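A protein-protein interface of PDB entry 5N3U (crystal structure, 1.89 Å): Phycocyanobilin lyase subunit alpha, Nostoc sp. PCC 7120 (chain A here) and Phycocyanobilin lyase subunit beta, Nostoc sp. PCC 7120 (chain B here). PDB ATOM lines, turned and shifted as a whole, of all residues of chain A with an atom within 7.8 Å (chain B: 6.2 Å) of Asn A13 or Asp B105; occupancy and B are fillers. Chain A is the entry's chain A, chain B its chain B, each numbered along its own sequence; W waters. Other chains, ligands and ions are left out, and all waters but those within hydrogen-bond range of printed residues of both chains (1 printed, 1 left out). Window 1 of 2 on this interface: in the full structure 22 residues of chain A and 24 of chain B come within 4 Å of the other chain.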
ATOM      1  N   PRO A  10      10.353  16.555 -14.288  1.00  0.00           N
ATOM      2  CA  PRO A  10      11.337  17.601 -14.428  1.00  0.00           C
ATOM      3  C   PRO A  10      12.158  17.608 -15.730  1.00  0.00           C
ATOM      4  O   PRO A  10      12.418  16.587 -16.301  1.00  0.00           O
ATOM      5  CB  PRO A  10      12.197  17.393 -13.190  1.00  0.00           C
ATOM      6  CG  PRO A  10      11.269  16.785 -12.200  1.00  0.00           C
ATOM      7  CD  PRO A  10      10.527  15.811 -13.029  1.00  0.00           C
ATOM      8  N   ALA A  11      12.531  18.816 -16.187  1.00  0.00           N
ATOM      9  CA  ALA A  11      13.532  19.013 -17.275  1.00  0.00           C
ATOM     10  C   ALA A  11      14.800  18.105 -17.105  1.00  0.00           C
ATOM     11  O   ALA A  11      15.124  17.321 -18.000  1.00  0.00           O
ATOM     12  CB  ALA A  11      13.930  20.491 -17.357  1.00  0.00           C
ATOM     13  N   GLU A  12      15.410  18.156 -15.908  1.00  0.00           N
ATOM     14  CA  GLU A  12      16.606  17.318 -15.490  1.00  0.00           C
ATOM     15  C   GLU A  12      16.335  16.224 -14.395  1.00  0.00           C
ATOM     16  O   GLU A  12      15.475  16.407 -13.554  1.00  0.00           O
ATOM     17  CB  GLU A  12      17.728  18.235 -14.953  1.00  0.00           C
ATOM     18  CG  GLU A  12      17.286  19.508 -14.226  1.00  0.00           C
ATOM     19  CD  GLU A  12      16.420  19.285 -12.977  1.00  0.00           C
ATOM     20  OE1 GLU A  12      16.835  18.516 -12.070  1.00  0.00           O
ATOM     21  OE2 GLU A  12      15.323  19.915 -12.881  1.00  0.00           O
ATOM     22  N   ASN A  13      17.034  15.084 -14.413  1.00  0.00           N
ATOM     23  CA  ASN A  13      17.163  14.216 -13.175  1.00  0.00           C
ATOM     24  C   ASN A  13      18.630  13.958 -12.860  1.00  0.00           C
ATOM     25  O   ASN A  13      18.980  12.973 -12.139  1.00  0.00           O
ATOM     26  CB  ASN A  13      16.375  12.865 -13.237  1.00  0.00           C
ATOM     27  CG  ASN A  13      17.152  11.703 -13.934  1.00  0.00           C
ATOM     28  OD1 ASN A  13      17.893  11.912 -14.871  1.00  0.00           O
ATOM     29  ND2 ASN A  13      16.929  10.506 -13.505  1.00  0.00           N
ATOM     30  N   GLY A  14      19.505  14.795 -13.431  1.00  0.00           N
ATOM     31  CA  GLY A  14      20.925  14.430 -13.424  1.00  0.00           C
ATOM     32  C   GLY A  14      21.766  15.220 -14.381  1.00  0.00           C
ATOM     33  O   GLY A  14      21.233  16.067 -15.057  1.00  0.00           O
ATOM     34  N   PRO A  15      23.092  14.965 -14.399  1.00  0.00           N
ATOM     35  CA  PRO A  15      23.943  15.670 -15.385  1.00  0.00           C
ATOM     36  C   PRO A  15      23.328  15.555 -16.797  1.00  0.00           C
ATOM     37  O   PRO A  15      22.644  14.569 -17.121  1.00  0.00           O
ATOM     38  CB  PRO A  15      25.340  14.991 -15.243  1.00  0.00           C
ATOM     39  CG  PRO A  15      25.169  13.820 -14.333  1.00  0.00           C
ATOM     40  CD  PRO A  15      23.885  14.051 -13.545  1.00  0.00           C
ATOM     41  N   GLN A  16      23.463  16.609 -17.579  1.00  0.00           N
ATOM     42  CA  GLN A  16      22.890  16.613 -18.914  1.00  0.00           C
ATOM     43  C   GLN A  16      23.945  15.903 -19.798  1.00  0.00           C
ATOM     44  O   GLN A  16      25.115  16.282 -19.806  1.00  0.00           O
ATOM     45  CB  GLN A  16      22.561  18.021 -19.408  1.00  0.00           C
ATOM     46  CG  GLN A  16      21.281  18.020 -20.274  1.00  0.00           C
ATOM     47  CD  GLN A  16      19.991  18.223 -19.456  1.00  0.00           C
ATOM     48  OE1 GLN A  16      19.788  19.295 -18.918  1.00  0.00           O
ATOM     49  NE2 GLN A  16      19.122  17.204 -19.372  1.00  0.00           N
ATOM     50  N   TYR A  36      25.253   6.217 -13.220  1.00  0.00           N
ATOM     51  CA  TYR A  36      24.222   7.001 -13.820  1.00  0.00           C
ATOM     52  C   TYR A  36      24.305   6.879 -15.320  1.00  0.00           C
ATOM     53  O   TYR A  36      23.315   6.659 -16.021  1.00  0.00           O
ATOM     54  CB  TYR A  36      24.338   8.459 -13.339  1.00  0.00           C
ATOM     55  CG  TYR A  36      23.223   9.276 -13.918  1.00  0.00           C
ATOM     56  CD1 TYR A  36      23.367   9.866 -15.130  1.00  0.00           C
ATOM     57  CD2 TYR A  36      22.011   9.403 -13.247  1.00  0.00           C
ATOM     58  CE1 TYR A  36      22.382  10.576 -15.704  1.00  0.00           C
ATOM     59  CE2 TYR A  36      20.972  10.131 -13.794  1.00  0.00           C
ATOM     60  CZ  TYR A  36      21.191  10.725 -15.024  1.00  0.00           C
ATOM     61  OH  TYR A  36      20.239  11.416 -15.605  1.00  0.00           O
ATOM     62  N   TRP A  39      22.843   3.622 -16.590  1.00  0.00           N
ATOM     63  CA  TRP A  39      21.383   3.741 -16.636  1.00  0.00           C
ATOM     64  C   TRP A  39      20.904   4.610 -17.790  1.00  0.00           C
ATOM     65  O   TRP A  39      19.994   4.263 -18.520  1.00  0.00           O
ATOM     66  CB  TRP A  39      20.881   4.322 -15.243  1.00  0.00           C
ATOM     67  CG  TRP A  39      19.463   4.669 -15.269  1.00  0.00           C
ATOM     68  CD1 TRP A  39      18.427   3.860 -14.982  1.00  0.00           C
ATOM     69  CD2 TRP A  39      18.911   5.919 -15.576  1.00  0.00           C
ATOM     70  NE1 TRP A  39      17.276   4.487 -15.203  1.00  0.00           N
ATOM     71  CE2 TRP A  39      17.510   5.759 -15.553  1.00  0.00           C
ATOM     72  CE3 TRP A  39      19.452   7.139 -15.933  1.00  0.00           C
ATOM     73  CZ2 TRP A  39      16.625   6.797 -15.807  1.00  0.00           C
ATOM     74  CZ3 TRP A  39      18.567   8.202 -16.205  1.00  0.00           C
ATOM     75  CH2 TRP A  39      17.164   8.005 -16.161  1.00  0.00           C
ATOM     76  N   TRP A  40      21.564   5.770 -18.002  1.00  0.00           N
ATOM     77  CA  TRP A  40      21.151   6.681 -19.040  1.00  0.00           C
ATOM     78  C   TRP A  40      21.204   6.055 -20.424  1.00  0.00           C
ATOM     79  O   TRP A  40      20.304   6.253 -21.269  1.00  0.00           O
ATOM     80  CB  TRP A  40      21.991   7.931 -18.978  1.00  0.00           C
ATOM     81  CG  TRP A  40      21.553   9.080 -19.798  1.00  0.00           C
ATOM     82  CD1 TRP A  40      20.835  10.168 -19.410  1.00  0.00           C
ATOM     83  CD2 TRP A  40      21.946   9.336 -21.153  1.00  0.00           C
ATOM     84  NE1 TRP A  40      20.678  11.060 -20.471  1.00  0.00           N
ATOM     85  CE2 TRP A  40      21.338  10.549 -21.555  1.00  0.00           C
ATOM     86  CE3 TRP A  40      22.697   8.624 -22.078  1.00  0.00           C
ATOM     87  CZ2 TRP A  40      21.506  11.088 -22.841  1.00  0.00           C
ATOM     88  CZ3 TRP A  40      22.843   9.158 -23.390  1.00  0.00           C
ATOM     89  CH2 TRP A  40      22.255  10.390 -23.735  1.00  0.00           C
ATOM     90  N   LYS A  43      18.194   3.816 -20.706  1.00  0.00           N
ATOM     91  CA  LYS A  43      16.965   4.551 -20.703  1.00  0.00           C
ATOM     92  C   LYS A  43      16.716   5.218 -22.053  1.00  0.00           C
ATOM     93  O   LYS A  43      15.612   5.219 -22.564  1.00  0.00           O
ATOM     94  CB  LYS A  43      17.083   5.581 -19.606  1.00  0.00           C
ATOM     95  CG  LYS A  43      15.965   6.636 -19.559  1.00  0.00           C
ATOM     96  CD  LYS A  43      14.597   6.049 -19.371  1.00  0.00           C
ATOM     97  CE  LYS A  43      13.695   7.270 -19.196  1.00  0.00           C
ATOM     98  NZ  LYS A  43      12.377   6.841 -18.760  1.00  0.00           N
ATOM     99  N   TYR A  44      17.752   5.818 -22.630  1.00  0.00           N
ATOM    100  CA  TYR A  44      17.653   6.504 -23.915  1.00  0.00           C
ATOM    101  C   TYR A  44      17.947   5.570 -25.064  1.00  0.00           C
ATOM    102  O   TYR A  44      17.974   6.000 -26.225  1.00  0.00           O
ATOM    103  CB  TYR A  44      18.566   7.766 -23.916  1.00  0.00           C
ATOM    104  CG  TYR A  44      18.010   8.763 -22.952  1.00  0.00           C
ATOM    105  CD1 TYR A  44      18.302   8.673 -21.606  1.00  0.00           C
ATOM    106  CD2 TYR A  44      17.156   9.764 -23.378  1.00  0.00           C
ATOM    107  CE1 TYR A  44      17.768   9.545 -20.674  1.00  0.00           C
ATOM    108  CE2 TYR A  44      16.575  10.633 -22.448  1.00  0.00           C
ATOM    109  CZ  TYR A  44      16.861  10.487 -21.089  1.00  0.00           C
ATOM    110  OH  TYR A  44      16.316  11.303 -20.090  1.00  0.00           O
ATOM    111  N   ASP B  73       6.722   0.723  -9.509  1.00  0.00           N
ATOM    112  CA  ASP B  73       7.524   1.437 -10.556  1.00  0.00           C
ATOM    113  C   ASP B  73       6.708   2.180 -11.549  1.00  0.00           C
ATOM    114  O   ASP B  73       7.271   2.779 -12.413  1.00  0.00           O
ATOM    115  CB  ASP B  73       8.473   0.468 -11.262  1.00  0.00           C
ATOM    116  CG  ASP B  73       9.626   0.060 -10.333  1.00  0.00           C
ATOM    117  OD1 ASP B  73       9.996   0.910  -9.504  1.00  0.00           O
ATOM    118  OD2 ASP B  73      10.058  -1.083 -10.380  1.00  0.00           O
ATOM    119  N   TYR B  76       4.525   7.126  -9.182  1.00  0.00           N
ATOM    120  CA  TYR B  76       5.494   7.815  -8.384  1.00  0.00           C
ATOM    121  C   TYR B  76       4.910   8.195  -7.009  1.00  0.00           C
ATOM    122  O   TYR B  76       5.665   8.274  -6.048  1.00  0.00           O
ATOM    123  CB  TYR B  76       6.114   9.027  -9.073  1.00  0.00           C
ATOM    124  CG  TYR B  76       5.214  10.197  -9.308  1.00  0.00           C
ATOM    125  CD1 TYR B  76       4.923  11.075  -8.295  1.00  0.00           C
ATOM    126  CD2 TYR B  76       4.611  10.406 -10.575  1.00  0.00           C
ATOM    127  CE1 TYR B  76       4.042  12.158  -8.485  1.00  0.00           C
ATOM    128  CE2 TYR B  76       3.751  11.484 -10.773  1.00  0.00           C
ATOM    129  CZ  TYR B  76       3.436  12.313  -9.714  1.00  0.00           C
ATOM    130  OH  TYR B  76       2.630  13.369  -9.934  1.00  0.00           O
ATOM    131  N   ARG B  79       5.270   5.180  -4.921  1.00  0.00           N
ATOM    132  CA  ARG B  79       6.664   4.863  -4.757  1.00  0.00           C
ATOM    133  C   ARG B  79       7.322   5.716  -3.692  1.00  0.00           C
ATOM    134  O   ARG B  79       8.187   5.230  -2.944  1.00  0.00           O
ATOM    135  CB  ARG B  79       7.352   4.958  -6.133  1.00  0.00           C
ATOM    136  CG  ARG B  79       8.773   4.549  -6.129  1.00  0.00           C
ATOM    137  CD  ARG B  79       9.282   4.207  -7.557  1.00  0.00           C
ATOM    138  NE  ARG B  79       9.399   5.377  -8.424  1.00  0.00           N
ATOM    139  CZ  ARG B  79       8.549   5.750  -9.407  1.00  0.00           C
ATOM    140  NH1 ARG B  79       8.817   6.840 -10.093  1.00  0.00           N
ATOM    141  NH2 ARG B  79       7.405   5.074  -9.676  1.00  0.00           N
ATOM    142  N   ASP B 100      19.226   3.899  -5.917  1.00  0.00           N
ATOM    143  CA  ASP B 100      18.582   3.970  -7.188  1.00  0.00           C
ATOM    144  C   ASP B 100      17.564   5.036  -7.289  1.00  0.00           C
ATOM    145  O   ASP B 100      17.480   5.727  -8.282  1.00  0.00           O
ATOM    146  CB  ASP B 100      17.826   2.654  -7.468  1.00  0.00           C
ATOM    147  CG  ASP B 100      18.700   1.662  -8.069  1.00  0.00           C
ATOM    148  OD1 ASP B 100      19.797   2.067  -8.509  1.00  0.00           O
ATOM    149  OD2 ASP B 100      18.348   0.454  -8.117  1.00  0.00           O
ATOM    150  N   ALA B 101      16.734   5.150  -6.282  1.00  0.00           N
ATOM    151  CA  ALA B 101      15.746   6.147  -6.195  1.00  0.00           C
ATOM    152  C   ALA B 101      16.301   7.525  -6.155  1.00  0.00           C
ATOM    153  O   ALA B 101      15.874   8.373  -6.894  1.00  0.00           O
ATOM    154  CB  ALA B 101      14.925   5.937  -4.940  1.00  0.00           C
ATOM    155  N   ALA B 102      17.304   7.760  -5.341  1.00  0.00           N
ATOM    156  CA  ALA B 102      17.932   9.057  -5.297  1.00  0.00           C
ATOM    157  C   ALA B 102      18.612   9.457  -6.591  1.00  0.00           C
ATOM    158  O   ALA B 102      18.537  10.602  -7.006  1.00  0.00           O
ATOM    159  CB  ALA B 102      18.905   9.096  -4.179  1.00  0.00           C
ATOM    160  N   ALA B 103      19.317   8.527  -7.210  1.00  0.00           N
ATOM    161  CA  ALA B 103      20.148   8.807  -8.383  1.00  0.00           C
ATOM    162  C   ALA B 103      19.437   8.783  -9.724  1.00  0.00           C
ATOM    163  O   ALA B 103      19.833   9.540 -10.631  1.00  0.00           O
ATOM    164  CB  ALA B 103      21.340   7.819  -8.416  1.00  0.00           C
ATOM    165  N   THR B 104      18.434   7.901  -9.926  1.00  0.00           N
ATOM    166  CA  THR B 104      17.879   7.697 -11.247  1.00  0.00           C
ATOM    167  C   THR B 104      16.383   7.861 -11.375  1.00  0.00           C
ATOM    168  O   THR B 104      15.871   7.895 -12.489  1.00  0.00           O
ATOM    169  CB  THR B 104      18.281   6.359 -11.832  1.00  0.00           C
ATOM    170  OG1 THR B 104      17.810   5.293 -10.992  1.00  0.00           O
ATOM    171  CG2 THR B 104      19.871   6.238 -11.928  1.00  0.00           C
ATOM    172  N   ASP B 105      15.660   7.979 -10.282  1.00  0.00           N
ATOM    173  CA  ASP B 105      14.240   8.266 -10.384  1.00  0.00           C
ATOM    174  C   ASP B 105      14.013   9.659 -10.931  1.00  0.00           C
ATOM    175  O   ASP B 105      14.893  10.504 -10.790  1.00  0.00           O
ATOM    176  CB  ASP B 105      13.552   8.120  -8.984  1.00  0.00           C
ATOM    177  CG  ASP B 105      12.101   7.635  -9.159  1.00  0.00           C
ATOM    178  OD1 ASP B 105      11.260   8.410  -9.660  1.00  0.00           O
ATOM    179  OD2 ASP B 105      11.807   6.470  -8.804  1.00  0.00           O
ATOM    180  N   PHE B 106      12.913   9.908 -11.627  1.00  0.00           N
ATOM    181  CA  PHE B 106      12.619  11.237 -12.103  1.00  0.00           C
ATOM    182  C   PHE B 106      11.745  12.012 -11.113  1.00  0.00           C
ATOM    183  O   PHE B 106      11.791  13.202 -11.109  1.00  0.00           O
ATOM    184  CB  PHE B 106      11.904  11.243 -13.432  1.00  0.00           C
ATOM    185  CG  PHE B 106      12.797  11.013 -14.599  1.00  0.00           C
ATOM    186  CD1 PHE B 106      13.538  12.075 -15.167  1.00  0.00           C
ATOM    187  CD2 PHE B 106      12.930   9.739 -15.141  1.00  0.00           C
ATOM    188  CE1 PHE B 106      14.400  11.852 -16.242  1.00  0.00           C
ATOM    189  CE2 PHE B 106      13.768   9.524 -16.230  1.00  0.00           C
ATOM    190  CZ  PHE B 106      14.506  10.583 -16.770  1.00  0.00           C
ATOM    191  N   ALA B 107      10.986  11.316 -10.249  1.00  0.00           N
ATOM    192  CA  ALA B 107      10.077  12.012  -9.373  1.00  0.00           C
ATOM    193  C   ALA B 107      10.749  12.664  -8.178  1.00  0.00           C
ATOM    194  O   ALA B 107      11.319  11.986  -7.351  1.00  0.00           O
ATOM    195  CB  ALA B 107       9.048  11.053  -8.892  1.00  0.00           C
ATOM    196  N   PRO B 108      10.626  14.000  -8.043  1.00  0.00           N
ATOM    197  CA  PRO B 108      11.254  14.664  -6.935  1.00  0.00           C
ATOM    198  C   PRO B 108      10.840  14.200  -5.562  1.00  0.00           C
ATOM    199  O   PRO B 108      11.706  14.085  -4.709  1.00  0.00           O
ATOM    200  CB  PRO B 108      10.860  16.120  -7.091  1.00  0.00           C
ATOM    201  CG  PRO B 108      10.650  16.315  -8.540  1.00  0.00           C
ATOM    202  CD  PRO B 108      10.092  14.942  -9.027  1.00  0.00           C
ATOM    203  N   VAL B 110      10.090  11.288  -4.761  1.00  0.00           N
ATOM    204  CA  VAL B 110      10.781  10.009  -4.514  1.00  0.00           C
ATOM    205  C   VAL B 110      12.227  10.249  -4.162  1.00  0.00           C
ATOM    206  O   VAL B 110      12.750   9.656  -3.216  1.00  0.00           O
ATOM    207  CB  VAL B 110      10.673   9.100  -5.721  1.00  0.00           C
ATOM    208  CG1 VAL B 110      11.628   7.890  -5.591  1.00  0.00           C
ATOM    209  CG2 VAL B 110       9.273   8.640  -5.887  1.00  0.00           C
ATOM    210  N   ARG B 111      12.914  11.043  -4.960  1.00  0.00           N
ATOM    211  CA  ARG B 111      14.307  11.337  -4.754  1.00  0.00           C
ATOM    212  C   ARG B 111      14.603  11.987  -3.387  1.00  0.00           C
ATOM    213  O   ARG B 111      15.634  11.672  -2.763  1.00  0.00           O
ATOM    214  CB  ARG B 111      14.810  12.242  -5.896  1.00  0.00           C
ATOM    215  CG  ARG B 111      14.641  11.653  -7.299  1.00  0.00           C
ATOM    216  CD  ARG B 111      15.202  12.521  -8.418  1.00  0.00           C
ATOM    217  NE  ARG B 111      16.649  12.472  -8.302  1.00  0.00           N
ATOM    218  CZ  ARG B 111      17.477  13.351  -8.826  1.00  0.00           C
ATOM    219  NH1 ARG B 111      17.045  14.370  -9.577  1.00  0.00           N
ATOM    220  NH2 ARG B 111      18.753  13.189  -8.602  1.00  0.00           N
ATOM    221  N   PHE B 144      26.944  12.998  -5.263  1.00  0.00           N
ATOM    222  CA  PHE B 144      26.486  13.119  -6.624  1.00  0.00           C
ATOM    223  C   PHE B 144      25.176  13.891  -6.798  1.00  0.00           C
ATOM    224  O   PHE B 144      25.068  14.756  -7.699  1.00  0.00           O
ATOM    225  CB  PHE B 144      26.452  11.720  -7.242  1.00  0.00           C
ATOM    226  CG  PHE B 144      25.877  11.647  -8.592  1.00  0.00           C
ATOM    227  CD1 PHE B 144      26.656  11.941  -9.668  1.00  0.00           C
ATOM    228  CD2 PHE B 144      24.605  11.132  -8.809  1.00  0.00           C
ATOM    229  CE1 PHE B 144      26.166  11.840 -10.922  1.00  0.00           C
ATOM    230  CE2 PHE B 144      24.078  11.055 -10.129  1.00  0.00           C
ATOM    231  CZ  PHE B 144      24.876  11.367 -11.179  1.00  0.00           C
ATOM    232  N   ASP B 148      22.470  18.380  -8.365  1.00  0.00           N
ATOM    233  CA  ASP B 148      21.307  18.467  -9.195  1.00  0.00           C
ATOM    234  C   ASP B 148      20.911  19.934  -9.370  1.00  0.00           C
ATOM    235  O   ASP B 148      21.131  20.754  -8.484  1.00  0.00           O
ATOM    236  CB  ASP B 148      20.127  17.731  -8.547  1.00  0.00           C
ATOM    237  CG  ASP B 148      19.071  17.375  -9.509  1.00  0.00           C
ATOM    238  OD1 ASP B 148      19.190  16.300 -10.177  1.00  0.00           O
ATOM    239  OD2 ASP B 148      18.081  18.124  -9.617  1.00  0.00           O
HETATM  240  O   HOH W   1      14.220  14.841 -10.971  1.00  0.00           O
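The side-chain amide nitrogen of Asn A13 sits at hydrogen-bond distance from the backbone carbonyl oxygen of Thr B104 (3.0 Å).
The side-chain amide nitrogen of Asn A13 is in hydrogen-bond range of the backbone carbonyl oxygen of Asp B105 (3.4 Å).
The side-chain carboxylate (OE1) of Glu A12 sits close to the side-chain carboxylate (OD2) of Asp B148, at 2.8 Å.
OH of Tyr A36 is in hydrogen-bond range of OD1 of Asn A13 (2.5 Å).
The guanidinium group of Arg B79 is in salt-bridge range of the side-chain carboxylate of Asp B105 (2.7 Å).
O of Asp B100 sits at hydrogen-bond distance from OG1 of Thr B104 (2.8 Å).
NE of Arg B111 lies within hydrogen-bond range of O of Ala B102.
The backbone NH (N) of Ala B107 sits at hydrogen-bond distance from the side-chain carboxylate (OD1) of Asp B105 (3.0 Å).
The guanidinium group (NH1) of Arg B111 lies within salt-bridge range of the side-chain carboxylate (OD1) of Asp B148, at 2.9 Å.
Among the printed residues, merely in contact across the chains: Pro A10 with Phe B106, Pro A10 with Pro B108, Asn A13 with Ala B103, Asn A13 with Phe B106, Asn A13 with Arg B111, Asn A13 with Asp B148, Gly A14 with Asp B148, Pro A15 with Phe B144, Tyr A36 with Ala B103, Tyr A36 with Phe B144, Trp A39 with Thr B104, Trp A39 with Phe B106, Lys A43 with Phe B106 and Tyr A44 with Phe B106.
Asn A13 touches six residues of chain B.
Asp B105 touches just one residue of chain A: Asn A13.
Printed residues of chain B within 4 Å of Glu A12: Asp B148.
Of the printed residues of chain A, Ala B103 touches Asn A13 and Tyr A36.
Of the printed residues of chain A, Arg B111 touches Asn A13.
The nearest residue of chain A that does not touch Asp B105 is Trp A39 (5.7 Å).
The nearest printed residue of chain A that does not touch Asp B148 is Pro A15 (5.9 Å).
Of the 16 printed residues of chain B, 8 touch a printed residue of chain A.
Hydrophobic or aromatic side chains of chain A within 4 Å of the printed part of chain B: Pro A10, Pro A15, Tyr A36, Trp A39 and Tyr A44.
Among the printed residues, no Asp or Glu carboxylate lies within 4 Å of a Lys or Arg side-chain nitrogen of the other chain.
Water W1 lies within hydrogen-bond range of O of Phe B106 (2.9 Å), NH1 of Arg B111 (3.2 Å) and O of Glu A12 (3.3 Å).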
